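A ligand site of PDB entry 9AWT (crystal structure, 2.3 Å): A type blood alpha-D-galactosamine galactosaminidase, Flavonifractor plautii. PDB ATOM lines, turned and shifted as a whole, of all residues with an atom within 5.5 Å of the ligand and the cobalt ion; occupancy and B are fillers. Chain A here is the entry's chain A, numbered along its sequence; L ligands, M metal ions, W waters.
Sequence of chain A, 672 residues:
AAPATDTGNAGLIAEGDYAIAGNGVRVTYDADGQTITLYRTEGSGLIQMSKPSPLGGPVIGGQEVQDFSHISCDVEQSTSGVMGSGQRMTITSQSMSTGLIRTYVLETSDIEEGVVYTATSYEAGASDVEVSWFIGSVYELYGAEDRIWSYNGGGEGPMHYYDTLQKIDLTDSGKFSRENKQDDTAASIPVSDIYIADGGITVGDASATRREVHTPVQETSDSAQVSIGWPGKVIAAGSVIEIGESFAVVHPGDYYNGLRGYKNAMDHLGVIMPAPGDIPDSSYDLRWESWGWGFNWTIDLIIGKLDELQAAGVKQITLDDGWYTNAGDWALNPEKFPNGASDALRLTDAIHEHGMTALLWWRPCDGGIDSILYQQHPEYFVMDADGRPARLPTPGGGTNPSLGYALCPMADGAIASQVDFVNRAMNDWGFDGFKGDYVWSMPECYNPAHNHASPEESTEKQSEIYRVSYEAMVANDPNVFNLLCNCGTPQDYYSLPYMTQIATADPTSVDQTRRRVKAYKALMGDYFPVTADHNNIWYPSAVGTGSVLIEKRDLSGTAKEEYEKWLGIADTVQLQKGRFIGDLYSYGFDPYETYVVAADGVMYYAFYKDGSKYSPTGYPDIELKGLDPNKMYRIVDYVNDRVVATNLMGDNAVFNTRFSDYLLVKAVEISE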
ATOM      1  N   MET A 159       7.597  31.188 -35.294  1.00  0.00           N
ATOM      2  CA  MET A 159       7.622  30.057 -34.370  1.00  0.00           C
ATOM      3  C   MET A 159       6.525  29.045 -34.718  1.00  0.00           C
ATOM      4  O   MET A 159       5.403  29.445 -35.002  1.00  0.00           O
ATOM      5  CB  MET A 159       7.251  30.490 -32.954  1.00  0.00           C
ATOM      6  CG  MET A 159       8.224  31.382 -32.281  1.00  0.00           C
ATOM      7  SD  MET A 159       7.858  31.620 -30.519  1.00  0.00           S
ATOM      8  CE  MET A 159       7.758  29.978 -29.773  1.00  0.00           C
ATOM      9  N   HIS A 160       6.866  27.750 -34.633  1.00  0.00           N
ATOM     10  CA  HIS A 160       5.909  26.654 -34.457  1.00  0.00           C
ATOM     11  C   HIS A 160       5.225  26.231 -35.758  1.00  0.00           C
ATOM     12  O   HIS A 160       5.232  25.050 -36.072  1.00  0.00           O
ATOM     13  CB  HIS A 160       4.863  26.942 -33.374  1.00  0.00           C
ATOM     14  CG  HIS A 160       5.357  26.926 -31.967  1.00  0.00           C
ATOM     15  ND1 HIS A 160       6.079  25.886 -31.415  1.00  0.00           N
ATOM     16  CD2 HIS A 160       5.163  27.814 -30.971  1.00  0.00           C
ATOM     17  CE1 HIS A 160       6.344  26.185 -30.133  1.00  0.00           C
ATOM     18  NE2 HIS A 160       5.810  27.353 -29.860  1.00  0.00           N
ATOM     19  N   GLU A 289       7.128  12.573 -19.285  1.00  0.00           N
ATOM     20  CA  GLU A 289       7.344  13.891 -18.705  1.00  0.00           C
ATOM     21  C   GLU A 289       6.034  14.362 -18.036  1.00  0.00           C
ATOM     22  O   GLU A 289       4.944  14.008 -18.499  1.00  0.00           O
ATOM     23  CB  GLU A 289       7.817  14.873 -19.789  1.00  0.00           C
ATOM     24  CG  GLU A 289       9.048  14.414 -20.575  1.00  0.00           C
ATOM     25  CD  GLU A 289       9.821  15.499 -21.332  1.00  0.00           C
ATOM     26  OE1 GLU A 289      11.081  15.505 -21.290  1.00  0.00           O
ATOM     27  OE2 GLU A 289       9.170  16.360 -21.974  1.00  0.00           O
ATOM     28  N   TRP A 291       4.415  17.103 -18.086  1.00  0.00           N
ATOM     29  CA  TRP A 291       3.859  18.323 -18.679  1.00  0.00           C
ATOM     30  C   TRP A 291       2.377  18.169 -19.030  1.00  0.00           C
ATOM     31  O   TRP A 291       1.714  19.162 -19.344  1.00  0.00           O
ATOM     32  CB  TRP A 291       4.631  18.785 -19.932  1.00  0.00           C
ATOM     33  CG  TRP A 291       4.170  20.089 -20.532  1.00  0.00           C
ATOM     34  CD1 TRP A 291       3.970  20.388 -21.853  1.00  0.00           C
ATOM     35  CD2 TRP A 291       3.888  21.323 -19.813  1.00  0.00           C
ATOM     36  NE1 TRP A 291       3.559  21.684 -22.012  1.00  0.00           N
ATOM     37  CE2 TRP A 291       3.509  22.286 -20.781  1.00  0.00           C
ATOM     38  CE3 TRP A 291       3.919  21.699 -18.458  1.00  0.00           C
ATOM     39  CZ2 TRP A 291       3.171  23.592 -20.420  1.00  0.00           C
ATOM     40  CZ3 TRP A 291       3.600  22.990 -18.117  1.00  0.00           C
ATOM     41  CH2 TRP A 291       3.230  23.921 -19.084  1.00  0.00           C
ATOM     42  N   PHE A 295       0.808  23.026 -14.872  1.00  0.00           N
ATOM     43  CA  PHE A 295       1.388  23.529 -13.641  1.00  0.00           C
ATOM     44  C   PHE A 295       0.763  22.845 -12.418  1.00  0.00           C
ATOM     45  O   PHE A 295       1.181  23.151 -11.300  1.00  0.00           O
ATOM     46  CB  PHE A 295       1.263  25.050 -13.605  1.00  0.00           C
ATOM     47  CG  PHE A 295       2.085  25.741 -14.694  1.00  0.00           C
ATOM     48  CD1 PHE A 295       3.479  25.649 -14.678  1.00  0.00           C
ATOM     49  CD2 PHE A 295       1.474  26.452 -15.719  1.00  0.00           C
ATOM     50  CE1 PHE A 295       4.232  26.274 -15.661  1.00  0.00           C
ATOM     51  CE2 PHE A 295       2.241  27.074 -16.701  1.00  0.00           C
ATOM     52  CZ  PHE A 295       3.621  26.985 -16.672  1.00  0.00           C
ATOM     53  N   ASP A 320       8.850  18.614 -15.230  1.00  0.00           N
ATOM     54  CA  ASP A 320       8.738  19.689 -16.205  1.00  0.00           C
ATOM     55  C   ASP A 320       8.498  21.026 -15.509  1.00  0.00           C
ATOM     56  O   ASP A 320       8.753  21.172 -14.321  1.00  0.00           O
ATOM     57  CB  ASP A 320       7.721  19.345 -17.288  1.00  0.00           C
ATOM     58  CG  ASP A 320       8.073  19.842 -18.686  1.00  0.00           C
ATOM     59  OD1 ASP A 320       7.788  20.998 -19.019  1.00  0.00           O
ATOM     60  OD2 ASP A 320       8.683  19.075 -19.443  1.00  0.00           O
ATOM     61  N   ASP A 321       7.981  21.991 -16.270  1.00  0.00           N
ATOM     62  CA  ASP A 321       7.850  23.381 -15.854  1.00  0.00           C
ATOM     63  C   ASP A 321       6.927  23.476 -14.640  1.00  0.00           C
ATOM     64  O   ASP A 321       5.995  22.660 -14.486  1.00  0.00           O
ATOM     65  CB  ASP A 321       7.367  24.236 -17.028  1.00  0.00           C
ATOM     66  CG  ASP A 321       7.569  25.748 -16.922  1.00  0.00           C
ATOM     67  OD1 ASP A 321       8.092  26.216 -15.862  1.00  0.00           O
ATOM     68  OD2 ASP A 321       7.208  26.463 -17.902  1.00  0.00           O
ATOM     69  N   TRP A 361      13.616  20.382 -15.726  1.00  0.00           N
ATOM     70  CA  TRP A 361      13.347  21.479 -16.637  1.00  0.00           C
ATOM     71  C   TRP A 361      14.069  22.749 -16.156  1.00  0.00           C
ATOM     72  O   TRP A 361      14.072  23.014 -14.954  1.00  0.00           O
ATOM     73  CB  TRP A 361      11.824  21.716 -16.705  1.00  0.00           C
ATOM     74  CG  TRP A 361      11.340  22.718 -17.720  1.00  0.00           C
ATOM     75  CD1 TRP A 361      10.820  22.418 -18.948  1.00  0.00           C
ATOM     76  CD2 TRP A 361      11.306  24.163 -17.629  1.00  0.00           C
ATOM     77  NE1 TRP A 361      10.461  23.559 -19.610  1.00  0.00           N
ATOM     78  CE2 TRP A 361      10.746  24.645 -18.828  1.00  0.00           C
ATOM     79  CE3 TRP A 361      11.697  25.092 -16.653  1.00  0.00           C
ATOM     80  CZ2 TRP A 361      10.576  26.005 -19.086  1.00  0.00           C
ATOM     81  CZ3 TRP A 361      11.516  26.433 -16.904  1.00  0.00           C
ATOM     82  CH2 TRP A 361      10.971  26.882 -18.109  1.00  0.00           C
ATOM     83  N   ASN A 400       8.061  37.757 -24.494  1.00  0.00           N
ATOM     84  CA  ASN A 400       7.035  36.877 -23.980  1.00  0.00           C
ATOM     85  C   ASN A 400       6.938  37.107 -22.476  1.00  0.00           C
ATOM     86  O   ASN A 400       7.958  37.287 -21.812  1.00  0.00           O
ATOM     87  CB  ASN A 400       7.360  35.450 -24.387  1.00  0.00           C
ATOM     88  CG  ASN A 400       6.440  34.418 -23.814  1.00  0.00           C
ATOM     89  OD1 ASN A 400       6.586  33.982 -22.668  1.00  0.00           O
ATOM     90  ND2 ASN A 400       5.537  33.936 -24.655  1.00  0.00           N
ATOM     91  N   LYS A 435      16.522  19.253 -19.043  1.00  0.00           N
ATOM     92  CA  LYS A 435      15.767  19.672 -20.199  1.00  0.00           C
ATOM     93  C   LYS A 435      15.739  21.194 -20.223  1.00  0.00           C
ATOM     94  O   LYS A 435      14.904  21.808 -19.568  1.00  0.00           O
ATOM     95  CB  LYS A 435      14.351  19.087 -20.157  1.00  0.00           C
ATOM     96  CG  LYS A 435      13.425  19.601 -21.251  1.00  0.00           C
ATOM     97  CD  LYS A 435      11.983  19.125 -21.157  1.00  0.00           C
ATOM     98  CE  LYS A 435      11.109  19.649 -22.257  1.00  0.00           C
ATOM     99  NZ  LYS A 435       9.705  19.228 -22.120  1.00  0.00           N
ATOM    100  N   ASP A 437      14.992  24.697 -22.154  1.00  0.00           N
ATOM    101  CA  ASP A 437      13.814  24.982 -22.946  1.00  0.00           C
ATOM    102  C   ASP A 437      13.423  26.462 -22.919  1.00  0.00           C
ATOM    103  O   ASP A 437      13.839  27.200 -22.036  1.00  0.00           O
ATOM    104  CB  ASP A 437      12.736  24.113 -22.343  1.00  0.00           C
ATOM    105  CG  ASP A 437      11.498  24.031 -23.189  1.00  0.00           C
ATOM    106  OD1 ASP A 437      11.604  23.483 -24.299  1.00  0.00           O
ATOM    107  OD2 ASP A 437      10.491  24.572 -22.701  1.00  0.00           O
ATOM    108  N   TYR A 438      12.594  26.869 -23.900  1.00  0.00           N
ATOM    109  CA  TYR A 438      11.840  28.114 -23.851  1.00  0.00           C
ATOM    110  C   TYR A 438      12.796  29.316 -23.875  1.00  0.00           C
ATOM    111  O   TYR A 438      12.601  30.289 -23.151  1.00  0.00           O
ATOM    112  CB  TYR A 438      10.938  28.063 -22.610  1.00  0.00           C
ATOM    113  CG  TYR A 438       9.633  28.862 -22.589  1.00  0.00           C
ATOM    114  CD1 TYR A 438       9.532  30.141 -23.125  1.00  0.00           C
ATOM    115  CD2 TYR A 438       8.483  28.345 -21.951  1.00  0.00           C
ATOM    116  CE1 TYR A 438       8.345  30.847 -23.060  1.00  0.00           C
ATOM    117  CE2 TYR A 438       7.297  29.061 -21.873  1.00  0.00           C
ATOM    118  CZ  TYR A 438       7.215  30.315 -22.442  1.00  0.00           C
ATOM    119  OH  TYR A 438       6.056  31.056 -22.399  1.00  0.00           O
ATOM    120  N   TRP A 440      15.655  31.524 -26.868  1.00  0.00           N
ATOM    121  CA  TRP A 440      16.064  31.675 -28.259  1.00  0.00           C
ATOM    122  C   TRP A 440      17.401  32.436 -28.339  1.00  0.00           C
ATOM    123  O   TRP A 440      18.403  31.912 -27.843  1.00  0.00           O
ATOM    124  CB  TRP A 440      14.902  32.261 -29.089  1.00  0.00           C
ATOM    125  CG  TRP A 440      13.705  31.349 -29.063  1.00  0.00           C
ATOM    126  CD1 TRP A 440      13.452  30.306 -29.894  1.00  0.00           C
ATOM    127  CD2 TRP A 440      12.628  31.335 -28.092  1.00  0.00           C
ATOM    128  NE1 TRP A 440      12.291  29.661 -29.536  1.00  0.00           N
ATOM    129  CE2 TRP A 440      11.772  30.267 -28.437  1.00  0.00           C
ATOM    130  CE3 TRP A 440      12.296  32.130 -26.985  1.00  0.00           C
ATOM    131  CZ2 TRP A 440      10.618  29.977 -27.707  1.00  0.00           C
ATOM    132  CZ3 TRP A 440      11.163  31.835 -26.262  1.00  0.00           C
ATOM    133  CH2 TRP A 440      10.329  30.773 -26.612  1.00  0.00           C
ATOM    134  N   CYS A 485      15.855  22.943 -26.090  1.00  0.00           N
ATOM    135  CA  CYS A 485      14.817  23.195 -27.095  1.00  0.00           C
ATOM    136  C   CYS A 485      14.606  24.697 -27.296  1.00  0.00           C
ATOM    137  O   CYS A 485      14.011  25.371 -26.456  1.00  0.00           O
ATOM    138  CB  CYS A 485      13.531  22.421 -26.751  1.00  0.00           C
ATOM    139  SG  CYS A 485      12.169  22.587 -27.950  1.00  0.00           S
ATOM    140  N   ASN A 486      15.124  25.220 -28.419  1.00  0.00           N
ATOM    141  CA  ASN A 486      14.778  26.546 -28.916  1.00  0.00           C
ATOM    142  C   ASN A 486      13.439  26.415 -29.651  1.00  0.00           C
ATOM    143  O   ASN A 486      13.363  26.438 -30.893  1.00  0.00           O
ATOM    144  CB  ASN A 486      15.906  27.123 -29.783  1.00  0.00           C
ATOM    145  CG  ASN A 486      17.261  27.055 -29.133  1.00  0.00           C
ATOM    146  OD1 ASN A 486      18.116  26.261 -29.533  1.00  0.00           O
ATOM    147  ND2 ASN A 486      17.508  27.880 -28.125  1.00  0.00           N
ATOM    148  N   CYS A 487      12.390  26.239 -28.850  1.00  0.00           N
ATOM    149  CA  CYS A 487      11.116  25.686 -29.285  1.00  0.00           C
ATOM    150  C   CYS A 487      10.575  26.366 -30.554  1.00  0.00           C
ATOM    151  O   CYS A 487      10.493  27.592 -30.613  1.00  0.00           O
ATOM    152  CB  CYS A 487      10.027  25.931 -28.239  1.00  0.00           C
ATOM    153  SG  CYS A 487      10.507  25.763 -26.486  1.00  0.00           S
ATOM    154  N   ALA A 505      11.360  19.807 -31.528  1.00  0.00           N
ATOM    155  CA  ALA A 505      11.229  21.131 -30.905  1.00  0.00           C
ATOM    156  C   ALA A 505       9.831  21.728 -31.100  1.00  0.00           C
ATOM    157  O   ALA A 505       9.675  22.664 -31.867  1.00  0.00           O
ATOM    158  CB  ALA A 505      12.308  22.074 -31.390  1.00  0.00           C
ATOM    159  N   ASP A 506       8.841  21.203 -30.363  1.00  0.00           N
ATOM    160  CA  ASP A 506       7.450  21.627 -30.496  1.00  0.00           C
ATOM    161  C   ASP A 506       6.995  21.574 -31.949  1.00  0.00           C
ATOM    162  O   ASP A 506       6.420  22.525 -32.471  1.00  0.00           O
ATOM    163  CB  ASP A 506       7.204  22.994 -29.857  1.00  0.00           C
ATOM    164  CG  ASP A 506       7.193  23.036 -28.337  1.00  0.00           C
ATOM    165  OD1 ASP A 506       7.088  21.954 -27.667  1.00  0.00           O
ATOM    166  OD2 ASP A 506       7.263  24.177 -27.813  1.00  0.00           O
ATOM    167  N   ASP A 533       9.213  14.114 -30.039  1.00  0.00           N
ATOM    168  CA  ASP A 533       8.464  15.014 -29.136  1.00  0.00           C
ATOM    169  C   ASP A 533       7.034  14.477 -28.926  1.00  0.00           C
ATOM    170  O   ASP A 533       6.687  13.400 -29.420  1.00  0.00           O
ATOM    171  CB  ASP A 533       8.587  16.476 -29.577  1.00  0.00           C
ATOM    172  CG  ASP A 533       8.650  17.531 -28.463  1.00  0.00           C
ATOM    173  OD1 ASP A 533       8.088  17.301 -27.351  1.00  0.00           O
ATOM    174  OD2 ASP A 533       9.308  18.591 -28.699  1.00  0.00           O
ATOM    175  N   HIS A 534       6.206  15.205 -28.126  1.00  0.00           N
ATOM    176  CA  HIS A 534       4.927  14.688 -27.642  1.00  0.00           C
ATOM    177  C   HIS A 534       3.801  15.713 -27.777  1.00  0.00           C
ATOM    178  O   HIS A 534       2.745  15.574 -27.155  1.00  0.00           O
ATOM    179  CB  HIS A 534       5.048  14.152 -26.203  1.00  0.00           C
ATOM    180  CG  HIS A 534       5.759  15.061 -25.236  1.00  0.00           C
ATOM    181  ND1 HIS A 534       5.661  16.444 -25.244  1.00  0.00           N
ATOM    182  CD2 HIS A 534       6.597  14.744 -24.222  1.00  0.00           C
ATOM    183  CE1 HIS A 534       6.407  16.928 -24.261  1.00  0.00           C
ATOM    184  NE2 HIS A 534       7.000  15.915 -23.630  1.00  0.00           N
ATOM    185  N   ASN A 535       3.989  16.724 -28.639  1.00  0.00           N
ATOM    186  CA  ASN A 535       2.999  17.773 -28.813  1.00  0.00           C
ATOM    187  C   ASN A 535       1.697  17.204 -29.319  1.00  0.00           C
ATOM    188  O   ASN A 535       0.649  17.699 -28.923  1.00  0.00           O
ATOM    189  CB  ASN A 535       3.469  18.840 -29.786  1.00  0.00           C
ATOM    190  CG  ASN A 535       4.741  19.476 -29.297  1.00  0.00           C
ATOM    191  OD1 ASN A 535       5.818  18.860 -29.411  1.00  0.00           O
ATOM    192  ND2 ASN A 535       4.627  20.683 -28.748  1.00  0.00           N
HETATM  193  C1  LIG L   1       7.024  22.275 -22.073  1.00  0.00           C
HETATM  194  C2  LIG L   1       6.627  23.749 -21.961  1.00  0.00           C
HETATM  195  C3  LIG L   1       6.561  24.207 -20.506  1.00  0.00           C
HETATM  196  N1  LIG L   1       8.652  22.434 -25.541  1.00  0.00           N
HETATM  197  C4  LIG L   1       8.394  22.745 -24.110  1.00  0.00           C
HETATM  198  C5  LIG L   1       7.282  21.842 -23.535  1.00  0.00           C
HETATM  199  O1  LIG L   1       7.694  20.446 -23.677  1.00  0.00           O
HETATM  200  O2  LIG L   1       8.198  22.023 -21.233  1.00  0.00           O
HETATM  201  O3  LIG L   1       6.250  25.593 -20.402  1.00  0.00           O
HETATM  202  O4  LIG L   1       7.659  24.565 -22.557  1.00  0.00           O
HETATM  203  C6  LIG L   1       8.006  24.239 -23.935  1.00  0.00           C
HETATM  204  O5  LIG L   1       6.960  24.618 -24.859  1.00  0.00           O
HETATM  205  C7  LIG L   1       6.618  25.920 -25.065  1.00  0.00           C
HETATM  206  C8  LIG L   1       5.419  26.476 -24.578  1.00  0.00           C
HETATM  207  C9  LIG L   1       5.114  27.811 -24.841  1.00  0.00           C
HETATM  208  C10 LIG L   1       7.482  26.693 -25.801  1.00  0.00           C
HETATM  209  C11 LIG L   1       7.190  28.014 -26.076  1.00  0.00           C
HETATM  210  C12 LIG L   1       6.017  28.556 -25.602  1.00  0.00           C
HETATM  211  N2  LIG L   1       5.760  29.870 -25.897  1.00  0.00           N
HETATM  212  O6  LIG L   1       6.637  30.495 -26.734  1.00  0.00           O
HETATM  213  O7  LIG L   1       4.654  30.512 -25.360  1.00  0.00           O
HETATM  214 CO    CO M   1      10.858  23.717 -26.248  1.00  0.00          CO
HETATM  215  O   HOH W   1       6.792  19.753 -26.352  1.00  0.00           O
HETATM  216  O   HOH W   2      10.412  20.141 -26.421  1.00  0.00           O
HETATM  217  O   HOH W   3       4.201  26.845 -21.297  1.00  0.00           O
HETATM  218  O   HOH W   4       3.202  31.879 -23.374  1.00  0.00           O
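The side-chain carboxylate (OD2) of Asp 320 is in salt-bridge range of the side-chain amino group (NZ) of Lys 435.
The side-chain amide nitrogen (ND2) of Asn 535 sits at hydrogen-bond distance from the side-chain carboxylate (OD1) of Asp 506 (3.0 Å).
The side-chain carboxylate (OE2) of Glu 289 is in salt-bridge range of the side-chain amino group (NZ) of Lys 435, at 2.9 Å.
The side-chain carboxylate (OD2) of Asp 533 lies within hydrogen-bond range of the backbone NH (N) of Asp 506, 3.1 Å away.
NE2 of His 534 is in hydrogen-bond range of OE2 of Glu 289, at 2.8 Å.
OH of Tyr 438 sits at hydrogen-bond distance from OD1 of Asn 400, 3.0 Å away.
SG of Cys 487 lies close to N of Tyr 438, at 3.5 Å.
N of Tyr 438 sits at hydrogen-bond distance from O of Cys 485.
The cobalt ion is bound by SG of Cys 487 (2.1 Å), OD1 of Asp 437 (2.1 Å) and SG of Cys 485 (2.4 Å).
The cobalt ion has three donor atoms within binding distance.
Slightly farther from the cobalt ion lies N1 of the ligand (2.6 Å).
Asp 506 touches the cobalt ion (OD2 to CO, 3.9 Å).
Four residues have an atom within 4 Å of the cobalt ion: Asp 437, Cys 485, Cys 487 and Asp 506.
The nearest printed residue that does not touch the cobalt ion is Tyr 438 (4.3 Å).
Residues that only touch the ligand: Met 159 (3.3 Å), Trp 291 (3.4 Å), Asn 400 (3.6 Å), Trp 440 (3.7 Å) and His 534 (3.8 Å).
Of the 21 residues printed, 13 come within 4 Å of the ligand.
The nearest printed residue that does not touch the ligand is His 160 (4.1 Å).
OD1 of Asp 437 sits close to N1 of the ligand (3.4 Å).
NE1 of Trp 361 is in hydrogen-bond range of O2 of the ligand (3.2 Å).
NZ of Lys 435 lies within hydrogen-bond range of O1 of the ligand, at 2.8 Å.
The side-chain carboxylate (OD1) of Asp 320 is in hydrogen-bond range of an oxygen (O2) of the ligand (2.5 Å).
A nitrogen (N1) of the ligand is in salt-bridge range of the side-chain carboxylate of Asp 506 (2.7 Å).
O7 of the ligand sits at hydrogen-bond distance from OH of Tyr 438, 3.3 Å away.
OD2 of Asp 321 is in hydrogen-bond range of O3 of the ligand, at 2.8 Å.
Water W4 lies within hydrogen-bond range of an oxygen (O7) of the ligand, the side-chain hydroxyl of Tyr 438 and the side-chain amide nitrogen of Asn 400.
Water W2 lies within hydrogen-bond range of the side-chain carboxylate of Asp 533 (3.0 Å) and a nitrogen (N1) of the ligand (3.0 Å).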
